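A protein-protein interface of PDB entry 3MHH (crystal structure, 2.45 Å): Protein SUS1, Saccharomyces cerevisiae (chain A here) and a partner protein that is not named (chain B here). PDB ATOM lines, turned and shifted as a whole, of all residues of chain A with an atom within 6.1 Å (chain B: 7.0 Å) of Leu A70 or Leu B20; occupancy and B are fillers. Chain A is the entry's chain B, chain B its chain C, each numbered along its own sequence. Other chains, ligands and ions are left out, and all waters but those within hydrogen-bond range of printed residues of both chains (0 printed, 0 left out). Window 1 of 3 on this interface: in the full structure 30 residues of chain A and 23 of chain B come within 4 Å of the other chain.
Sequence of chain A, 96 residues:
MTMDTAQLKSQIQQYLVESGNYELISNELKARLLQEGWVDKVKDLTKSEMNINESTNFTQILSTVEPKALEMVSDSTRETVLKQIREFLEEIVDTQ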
ATOM      1  N   LEU A  29      -6.043 -11.980  -8.158  1.00  0.00           N
ATOM      2  CA  LEU A  29      -6.419 -11.838  -9.552  1.00  0.00           C
ATOM      3  C   LEU A  29      -6.340 -10.382  -9.953  1.00  0.00           C
ATOM      4  O   LEU A  29      -5.815 -10.046 -11.008  1.00  0.00           O
ATOM      5  CB  LEU A  29      -7.836 -12.364  -9.775  1.00  0.00           C
ATOM      6  CG  LEU A  29      -8.408 -12.116 -11.167  1.00  0.00           C
ATOM      7  CD1 LEU A  29      -7.582 -12.806 -12.228  1.00  0.00           C
ATOM      8  CD2 LEU A  29      -9.824 -12.595 -11.203  1.00  0.00           C
ATOM      9  N   LEU A  33      -3.899  -8.731 -12.784  1.00  0.00           N
ATOM     10  CA  LEU A  33      -4.479  -8.129 -13.973  1.00  0.00           C
ATOM     11  C   LEU A  33      -4.072  -6.654 -14.077  1.00  0.00           C
ATOM     12  O   LEU A  33      -3.806  -6.128 -15.162  1.00  0.00           O
ATOM     13  CB  LEU A  33      -5.996  -8.271 -13.938  1.00  0.00           C
ATOM     14  CG  LEU A  33      -6.518  -9.700 -14.087  1.00  0.00           C
ATOM     15  CD1 LEU A  33      -7.994  -9.771 -13.764  1.00  0.00           C
ATOM     16  CD2 LEU A  33      -6.264 -10.217 -15.477  1.00  0.00           C
ATOM     17  N   TRP A  38      -3.739  -5.288 -17.953  1.00  0.00           N
ATOM     18  CA  TRP A  38      -5.058  -5.678 -18.450  1.00  0.00           C
ATOM     19  C   TRP A  38      -6.173  -4.694 -18.081  1.00  0.00           C
ATOM     20  O   TRP A  38      -7.056  -4.421 -18.889  1.00  0.00           O
ATOM     21  CB  TRP A  38      -5.391  -7.065 -17.934  1.00  0.00           C
ATOM     22  CG  TRP A  38      -6.715  -7.593 -18.328  1.00  0.00           C
ATOM     23  CD1 TRP A  38      -6.982  -8.419 -19.363  1.00  0.00           C
ATOM     24  CD2 TRP A  38      -7.955  -7.403 -17.634  1.00  0.00           C
ATOM     25  NE1 TRP A  38      -8.319  -8.740 -19.386  1.00  0.00           N
ATOM     26  CE2 TRP A  38      -8.938  -8.122 -18.336  1.00  0.00           C
ATOM     27  CE3 TRP A  38      -8.331  -6.676 -16.504  1.00  0.00           C
ATOM     28  CZ2 TRP A  38     -10.266  -8.146 -17.940  1.00  0.00           C
ATOM     29  CZ3 TRP A  38      -9.646  -6.712 -16.106  1.00  0.00           C
ATOM     30  CH2 TRP A  38     -10.599  -7.437 -16.820  1.00  0.00           C
ATOM     31  N   VAL A  65     -17.277  -5.630 -25.534  1.00  0.00           N
ATOM     32  CA  VAL A  65     -16.067  -5.568 -24.733  1.00  0.00           C
ATOM     33  C   VAL A  65     -15.764  -6.876 -24.003  1.00  0.00           C
ATOM     34  O   VAL A  65     -14.650  -7.388 -24.077  1.00  0.00           O
ATOM     35  CB  VAL A  65     -16.155  -4.461 -23.686  1.00  0.00           C
ATOM     36  CG1 VAL A  65     -15.006  -4.610 -22.670  1.00  0.00           C
ATOM     37  CG2 VAL A  65     -16.136  -3.104 -24.362  1.00  0.00           C
ATOM     38  N   GLU A  66     -16.755  -7.402 -23.290  1.00  0.00           N
ATOM     39  CA  GLU A  66     -16.564  -8.563 -22.423  1.00  0.00           C
ATOM     40  C   GLU A  66     -15.886  -9.737 -23.125  1.00  0.00           C
ATOM     41  O   GLU A  66     -14.797 -10.140 -22.732  1.00  0.00           O
ATOM     42  CB  GLU A  66     -17.893  -9.003 -21.798  1.00  0.00           C
ATOM     43  CG  GLU A  66     -17.732  -9.905 -20.592  1.00  0.00           C
ATOM     44  CD  GLU A  66     -18.997 -10.010 -19.775  1.00  0.00           C
ATOM     45  OE1 GLU A  66     -20.026 -10.465 -20.321  1.00  0.00           O
ATOM     46  OE2 GLU A  66     -18.963  -9.630 -18.585  1.00  0.00           O
ATOM     47  N   PRO A  67     -16.514 -10.292 -24.167  1.00  0.00           N
ATOM     48  CA  PRO A  67     -15.826 -11.395 -24.874  1.00  0.00           C
ATOM     49  C   PRO A  67     -14.350 -11.091 -25.153  1.00  0.00           C
ATOM     50  O   PRO A  67     -13.474 -11.899 -24.836  1.00  0.00           O
ATOM     51  CB  PRO A  67     -16.596 -11.522 -26.188  1.00  0.00           C
ATOM     52  CG  PRO A  67     -17.924 -10.881 -25.930  1.00  0.00           C
ATOM     53  CD  PRO A  67     -17.709  -9.819 -24.890  1.00  0.00           C
ATOM     54  N   LYS A  68     -14.090  -9.919 -25.723  1.00  0.00           N
ATOM     55  CA  LYS A  68     -12.726  -9.488 -26.011  1.00  0.00           C
ATOM     56  C   LYS A  68     -11.884  -9.394 -24.735  1.00  0.00           C
ATOM     57  O   LYS A  68     -10.732  -9.832 -24.713  1.00  0.00           O
ATOM     58  CB  LYS A  68     -12.743  -8.127 -26.711  1.00  0.00           C
ATOM     59  CG  LYS A  68     -13.544  -8.101 -27.996  1.00  0.00           C
ATOM     60  CD  LYS A  68     -13.307  -6.807 -28.771  1.00  0.00           C
ATOM     61  CE  LYS A  68     -13.737  -6.940 -30.228  1.00  0.00           C
ATOM     62  NZ  LYS A  68     -13.102  -5.901 -31.092  1.00  0.00           N
ATOM     63  N   ALA A  69     -12.474  -8.832 -23.679  1.00  0.00           N
ATOM     64  CA  ALA A  69     -11.773  -8.602 -22.413  1.00  0.00           C
ATOM     65  C   ALA A  69     -11.383  -9.906 -21.728  1.00  0.00           C
ATOM     66  O   ALA A  69     -10.280 -10.024 -21.210  1.00  0.00           O
ATOM     67  CB  ALA A  69     -12.626  -7.743 -21.482  1.00  0.00           C
ATOM     68  N   LEU A  70     -12.294 -10.873 -21.708  1.00  0.00           N
ATOM     69  CA  LEU A  70     -11.992 -12.207 -21.180  1.00  0.00           C
ATOM     70  C   LEU A  70     -10.792 -12.816 -21.904  1.00  0.00           C
ATOM     71  O   LEU A  70      -9.935 -13.452 -21.289  1.00  0.00           O
ATOM     72  CB  LEU A  70     -13.201 -13.141 -21.320  1.00  0.00           C
ATOM     73  CG  LEU A  70     -14.377 -12.885 -20.377  1.00  0.00           C
ATOM     74  CD1 LEU A  70     -15.590 -13.712 -20.774  1.00  0.00           C
ATOM     75  CD2 LEU A  70     -13.980 -13.166 -18.932  1.00  0.00           C
ATOM     76  N   GLU A  71     -10.733 -12.596 -23.211  1.00  0.00           N
ATOM     77  CA  GLU A  71      -9.715 -13.203 -24.067  1.00  0.00           C
ATOM     78  C   GLU A  71      -8.329 -12.581 -23.848  1.00  0.00           C
ATOM     79  O   GLU A  71      -7.312 -13.239 -24.052  1.00  0.00           O
ATOM     80  CB  GLU A  71     -10.134 -13.060 -25.534  1.00  0.00           C
ATOM     81  CG  GLU A  71      -9.697 -14.204 -26.430  1.00  0.00           C
ATOM     82  CD  GLU A  71     -10.566 -14.340 -27.678  1.00  0.00           C
ATOM     83  OE1 GLU A  71     -11.268 -13.363 -28.036  1.00  0.00           O
ATOM     84  OE2 GLU A  71     -10.548 -15.425 -28.303  1.00  0.00           O
ATOM     85  N   MET A  72      -8.301 -11.322 -23.423  1.00  0.00           N
ATOM     86  CA  MET A  72      -7.040 -10.607 -23.181  1.00  0.00           C
ATOM     87  C   MET A  72      -6.328 -11.008 -21.879  1.00  0.00           C
ATOM     88  O   MET A  72      -5.176 -10.634 -21.670  1.00  0.00           O
ATOM     89  CB  MET A  72      -7.278  -9.092 -23.154  1.00  0.00           C
ATOM     90  CG  MET A  72      -7.797  -8.515 -24.455  1.00  0.00           C
ATOM     91  SD  MET A  72      -8.605  -6.929 -24.176  1.00  0.00           S
ATOM     92  CE  MET A  72      -7.181  -5.868 -23.960  1.00  0.00           C
ATOM     93  N   VAL A  73      -6.999 -11.740 -20.995  1.00  0.00           N
ATOM     94  CA  VAL A  73      -6.325 -12.230 -19.797  1.00  0.00           C
ATOM     95  C   VAL A  73      -5.142 -13.093 -20.212  1.00  0.00           C
ATOM     96  O   VAL A  73      -5.294 -14.028 -20.991  1.00  0.00           O
ATOM     97  CB  VAL A  73      -7.261 -13.073 -18.909  1.00  0.00           C
ATOM     98  CG1 VAL A  73      -6.538 -13.512 -17.649  1.00  0.00           C
ATOM     99  CG2 VAL A  73      -8.514 -12.297 -18.558  1.00  0.00           C
ATOM    100  N   ARG A  78      -4.434 -16.496 -16.006  1.00  0.00           N
ATOM    101  CA  ARG A  78      -5.559 -17.421 -16.070  1.00  0.00           C
ATOM    102  C   ARG A  78      -5.211 -18.754 -15.421  1.00  0.00           C
ATOM    103  O   ARG A  78      -5.909 -19.221 -14.526  1.00  0.00           O
ATOM    104  CB  ARG A  78      -5.972 -17.654 -17.526  1.00  0.00           C
ATOM    105  CG  ARG A  78      -7.236 -18.480 -17.677  1.00  0.00           C
ATOM    106  CD  ARG A  78      -7.651 -18.615 -19.132  1.00  0.00           C
ATOM    107  NE  ARG A  78      -7.843 -17.317 -19.772  1.00  0.00           N
ATOM    108  CZ  ARG A  78      -7.097 -16.863 -20.776  1.00  0.00           C
ATOM    109  NH1 ARG A  78      -6.112 -17.609 -21.265  1.00  0.00           N
ATOM    110  NH2 ARG A  78      -7.344 -15.671 -21.301  1.00  0.00           N
ATOM    111  N   ASN B  13     -13.310 -22.915 -13.351  1.00  0.00           N
ATOM    112  CA  ASN B  13     -13.472 -21.977 -14.454  1.00  0.00           C
ATOM    113  C   ASN B  13     -14.692 -21.097 -14.184  1.00  0.00           C
ATOM    114  O   ASN B  13     -14.655 -19.883 -14.383  1.00  0.00           O
ATOM    115  CB  ASN B  13     -13.600 -22.705 -15.792  1.00  0.00           C
ATOM    116  CG  ASN B  13     -12.259 -23.214 -16.311  1.00  0.00           C
ATOM    117  OD1 ASN B  13     -11.402 -22.430 -16.727  1.00  0.00           O
ATOM    118  ND2 ASN B  13     -12.077 -24.533 -16.303  1.00  0.00           N
ATOM    119  N   GLY B  14     -15.755 -21.707 -13.673  1.00  0.00           N
ATOM    120  CA  GLY B  14     -16.968 -20.966 -13.345  1.00  0.00           C
ATOM    121  C   GLY B  14     -16.717 -19.886 -12.308  1.00  0.00           C
ATOM    122  O   GLY B  14     -17.239 -18.774 -12.418  1.00  0.00           O
ATOM    123  N   ILE B  15     -15.924 -20.217 -11.292  1.00  0.00           N
ATOM    124  CA  ILE B  15     -15.570 -19.244 -10.256  1.00  0.00           C
ATOM    125  C   ILE B  15     -14.716 -18.126 -10.851  1.00  0.00           C
ATOM    126  O   ILE B  15     -14.976 -16.960 -10.609  1.00  0.00           O
ATOM    127  CB  ILE B  15     -14.843 -19.913  -9.083  1.00  0.00           C
ATOM    128  CG1 ILE B  15     -15.806 -20.835  -8.342  1.00  0.00           C
ATOM    129  CG2 ILE B  15     -14.255 -18.880  -8.118  1.00  0.00           C
ATOM    130  CD1 ILE B  15     -15.126 -21.674  -7.292  1.00  0.00           C
ATOM    131  N   LEU B  16     -13.733 -18.479 -11.668  1.00  0.00           N
ATOM    132  CA  LEU B  16     -12.879 -17.485 -12.285  1.00  0.00           C
ATOM    133  C   LEU B  16     -13.678 -16.560 -13.188  1.00  0.00           C
ATOM    134  O   LEU B  16     -13.423 -15.355 -13.226  1.00  0.00           O
ATOM    135  CB  LEU B  16     -11.752 -18.151 -13.090  1.00  0.00           C
ATOM    136  CG  LEU B  16     -10.806 -17.148 -13.769  1.00  0.00           C
ATOM    137  CD1 LEU B  16     -10.066 -16.363 -12.719  1.00  0.00           C
ATOM    138  CD2 LEU B  16      -9.823 -17.822 -14.749  1.00  0.00           C
ATOM    139  N   ASN B  17     -14.633 -17.134 -13.917  1.00  0.00           N
ATOM    140  CA  ASN B  17     -15.461 -16.391 -14.878  1.00  0.00           C
ATOM    141  C   ASN B  17     -16.362 -15.373 -14.167  1.00  0.00           C
ATOM    142  O   ASN B  17     -16.483 -14.219 -14.589  1.00  0.00           O
ATOM    143  CB  ASN B  17     -16.291 -17.395 -15.687  1.00  0.00           C
ATOM    144  CG  ASN B  17     -17.173 -16.736 -16.744  1.00  0.00           C
ATOM    145  OD1 ASN B  17     -18.397 -16.717 -16.603  1.00  0.00           O
ATOM    146  ND2 ASN B  17     -16.563 -16.235 -17.821  1.00  0.00           N
ATOM    147  N   ASN B  18     -16.974 -15.794 -13.066  1.00  0.00           N
ATOM    148  CA  ASN B  18     -17.698 -14.864 -12.205  1.00  0.00           C
ATOM    149  C   ASN B  18     -16.773 -13.710 -11.796  1.00  0.00           C
ATOM    150  O   ASN B  18     -17.131 -12.531 -11.935  1.00  0.00           O
ATOM    151  CB  ASN B  18     -18.231 -15.567 -10.949  1.00  0.00           C
ATOM    152  CG  ASN B  18     -19.520 -16.361 -11.206  1.00  0.00           C
ATOM    153  OD1 ASN B  18     -20.288 -16.635 -10.282  1.00  0.00           O
ATOM    154  ND2 ASN B  18     -19.750 -16.733 -12.446  1.00  0.00           N
ATOM    155  N   LEU B  19     -15.581 -14.045 -11.312  1.00  0.00           N
ATOM    156  CA  LEU B  19     -14.658 -13.014 -10.855  1.00  0.00           C
ATOM    157  C   LEU B  19     -14.312 -12.135 -12.039  1.00  0.00           C
ATOM    158  O   LEU B  19     -14.310 -10.898 -11.942  1.00  0.00           O
ATOM    159  CB  LEU B  19     -13.390 -13.625 -10.255  1.00  0.00           C
ATOM    160  CG  LEU B  19     -13.481 -14.211  -8.842  1.00  0.00           C
ATOM    161  CD1 LEU B  19     -12.315 -15.157  -8.558  1.00  0.00           C
ATOM    162  CD2 LEU B  19     -13.548 -13.119  -7.771  1.00  0.00           C
ATOM    163  N   LEU B  20     -14.045 -12.772 -13.175  1.00  0.00           N
ATOM    164  CA  LEU B  20     -13.610 -12.032 -14.354  1.00  0.00           C
ATOM    165  C   LEU B  20     -14.717 -11.125 -14.900  1.00  0.00           C
ATOM    166  O   LEU B  20     -14.480  -9.953 -15.158  1.00  0.00           O
ATOM    167  CB  LEU B  20     -13.088 -12.984 -15.429  1.00  0.00           C
ATOM    168  CG  LEU B  20     -11.666 -13.508 -15.218  1.00  0.00           C
ATOM    169  CD1 LEU B  20     -11.312 -14.561 -16.269  1.00  0.00           C
ATOM    170  CD2 LEU B  20     -10.663 -12.367 -15.251  1.00  0.00           C
ATOM    171  N   THR B  21     -15.926 -11.659 -15.050  1.00  0.00           N
ATOM    172  CA  THR B  21     -17.030 -10.888 -15.639  1.00  0.00           C
ATOM    173  C   THR B  21     -17.467  -9.731 -14.737  1.00  0.00           C
ATOM    174  O   THR B  21     -17.763  -8.636 -15.212  1.00  0.00           O
ATOM    175  CB  THR B  21     -18.251 -11.790 -16.030  1.00  0.00           C
ATOM    176  OG1 THR B  21     -18.582 -12.675 -14.955  1.00  0.00           O
ATOM    177  CG2 THR B  21     -17.932 -12.634 -17.273  1.00  0.00           C
ATOM    178  N   THR B  22     -17.467  -9.949 -13.433  1.00  0.00           N
ATOM    179  CA  THR B  22     -17.841  -8.888 -12.509  1.00  0.00           C
ATOM    180  C   THR B  22     -16.864  -7.713 -12.631  1.00  0.00           C
ATOM    181  O   THR B  22     -17.269  -6.550 -12.615  1.00  0.00           O
ATOM    182  CB  THR B  22     -17.868  -9.377 -11.038  1.00  0.00           C
ATOM    183  OG1 THR B  22     -18.775 -10.492 -10.897  1.00  0.00           O
ATOM    184  CG2 THR B  22     -18.288  -8.228 -10.117  1.00  0.00           C
ATOM    185  N   LEU B  23     -15.575  -8.020 -12.727  1.00  0.00           N
ATOM    186  CA  LEU B  23     -14.563  -6.985 -12.808  1.00  0.00           C
ATOM    187  C   LEU B  23     -14.626  -6.233 -14.144  1.00  0.00           C
ATOM    188  O   LEU B  23     -14.493  -5.007 -14.167  1.00  0.00           O
ATOM    189  CB  LEU B  23     -13.179  -7.583 -12.605  1.00  0.00           C
ATOM    190  CG  LEU B  23     -12.021  -6.588 -12.690  1.00  0.00           C
ATOM    191  CD1 LEU B  23     -12.163  -5.451 -11.648  1.00  0.00           C
ATOM    192  CD2 LEU B  23     -10.703  -7.328 -12.539  1.00  0.00           C
ATOM    193  N   ILE B  24     -14.809  -6.961 -15.251  1.00  0.00           N
ATOM    194  CA  ILE B  24     -15.025  -6.332 -16.556  1.00  0.00           C
ATOM    195  C   ILE B  24     -16.257  -5.402 -16.529  1.00  0.00           C
ATOM    196  O   ILE B  24     -16.214  -4.279 -17.030  1.00  0.00           O
ATOM    197  CB  ILE B  24     -15.272  -7.385 -17.652  1.00  0.00           C
ATOM    198  CG1 ILE B  24     -14.005  -8.214 -17.928  1.00  0.00           C
ATOM    199  CG2 ILE B  24     -15.720  -6.710 -18.932  1.00  0.00           C
ATOM    200  CD1 ILE B  24     -14.288  -9.504 -18.721  1.00  0.00           C
ATOM    201  N   GLN B  25     -17.353  -5.895 -15.957  1.00  0.00           N
ATOM    202  CA  GLN B  25     -18.618  -5.157 -15.908  1.00  0.00           C
ATOM    203  C   GLN B  25     -18.556  -3.940 -15.007  1.00  0.00           C
ATOM    204  O   GLN B  25     -19.304  -2.994 -15.199  1.00  0.00           O
ATOM    205  CB  GLN B  25     -19.768  -6.066 -15.474  1.00  0.00           C
ATOM    206  CG  GLN B  25     -20.156  -7.066 -16.533  1.00  0.00           C
ATOM    207  CD  GLN B  25     -20.946  -8.242 -15.996  1.00  0.00           C
ATOM    208  OE1 GLN B  25     -21.782  -8.092 -15.107  1.00  0.00           O
ATOM    209  NE2 GLN B  25     -20.730  -9.418 -16.583  1.00  0.00           N
ATOM    210  N   ASP B  26     -17.669  -3.978 -14.023  1.00  0.00           N
ATOM    211  CA  ASP B  26     -17.402  -2.833 -13.165  1.00  0.00           C
ATOM    212  C   ASP B  26     -16.662  -1.765 -13.965  1.00  0.00           C
ATOM    213  O   ASP B  26     -17.076  -0.603 -13.993  1.00  0.00           O
ATOM    214  CB  ASP B  26     -16.532  -3.272 -11.984  1.00  0.00           C
ATOM    215  CG  ASP B  26     -16.235  -2.154 -11.026  1.00  0.00           C
ATOM    216  OD1 ASP B  26     -16.983  -1.151 -11.014  1.00  0.00           O
ATOM    217  OD2 ASP B  26     -15.263  -2.295 -10.257  1.00  0.00           O
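Of the printed residues of chain B, Leu A33 touches Leu B23.
Printed residues of chain B within 4 Å of Leu A70: Leu B20 (3.6 Å) and Ile B24 (3.7 Å).
Of the printed residues of chain B, Arg A78 touches Leu B16 (3.96 Å).
Gly B14 touches none of the printed residues of chain A.
Ile B15 touches none of the printed residues of chain A.
Of the printed residues of chain A, Leu B20 touches Leu A70 and Val A73.
The nearest printed residue of chain B that does not touch Leu A70 is Asn B17 (4.004 Å).
The nearest printed residue of chain A that does not touch Leu B20 is Leu A33 (4.01 Å).
The nearest printed residue of chain A that does not touch Thr B21 is Leu A70 (4.3 Å).
Of the 13 printed residues of chain A, 8 touch a printed residue of chain B.
Hydrophobic or aromatic side chains of chain A within 4 Å of the printed part of chain B: Leu A29, Leu A33, Trp A38, Ala A69, Leu A70 and Val A73.
Among the printed residues, 12 pairs touch across the chains.
Among the printed residues, no Asp or Glu carboxylate lies within 4 Å of a Lys or Arg side-chain nitrogen of the other chain.
Among the printed residues, pairs that only touch across the chains: Leu A29 with Leu B19 (3.8 Å), Leu A33 with Leu B23 (3.8 Å), Trp A38 with Leu B23 (3.8 Å), Trp A38 with Ile B24 (3.7 Å), Glu A66 with Thr B21 (3.4 Å), Glu A66 with Ile B24 (3.9 Å), Ala A69 with Ile B24 (3.7 Å), Leu A70 with Leu B20 (3.6 Å), Leu A70 with Ile B24 (3.7 Å), Val A73 with Leu B20 (3.9 Å) and Arg A78 with Leu B16 (3.96 Å).
The side-chain amide nitrogen of Gln B25 lies within hydrogen-bond range of the side-chain carboxylate of Glu A66, at 2.7 Å.
The backbone carbonyl oxygen of Leu A33 sits at hydrogen-bond distance from the backbone NH of Trp A38 (2.9 Å).
O of Ala A69 is in hydrogen-bond range of NE1 of Trp A38 (3.0 Å).
The guanidinium group (NH2) of Arg A78 is in hydrogen-bond range of the backbone carbonyl oxygen (O) of Leu A70 (3.4 Å).
The backbone carbonyl oxygen (O) of Val A73 sits at hydrogen-bond distance from the guanidinium group (NH2) of Arg A78, 2.6 Å away.
The side-chain hydroxyl (OG1) of Thr B21 lies within hydrogen-bond range of the backbone carbonyl oxygen (O) of Asn B17, 2.6 Å away.
NE2 of Gln B25 lies close to O of Thr B21 (3.4 Å).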
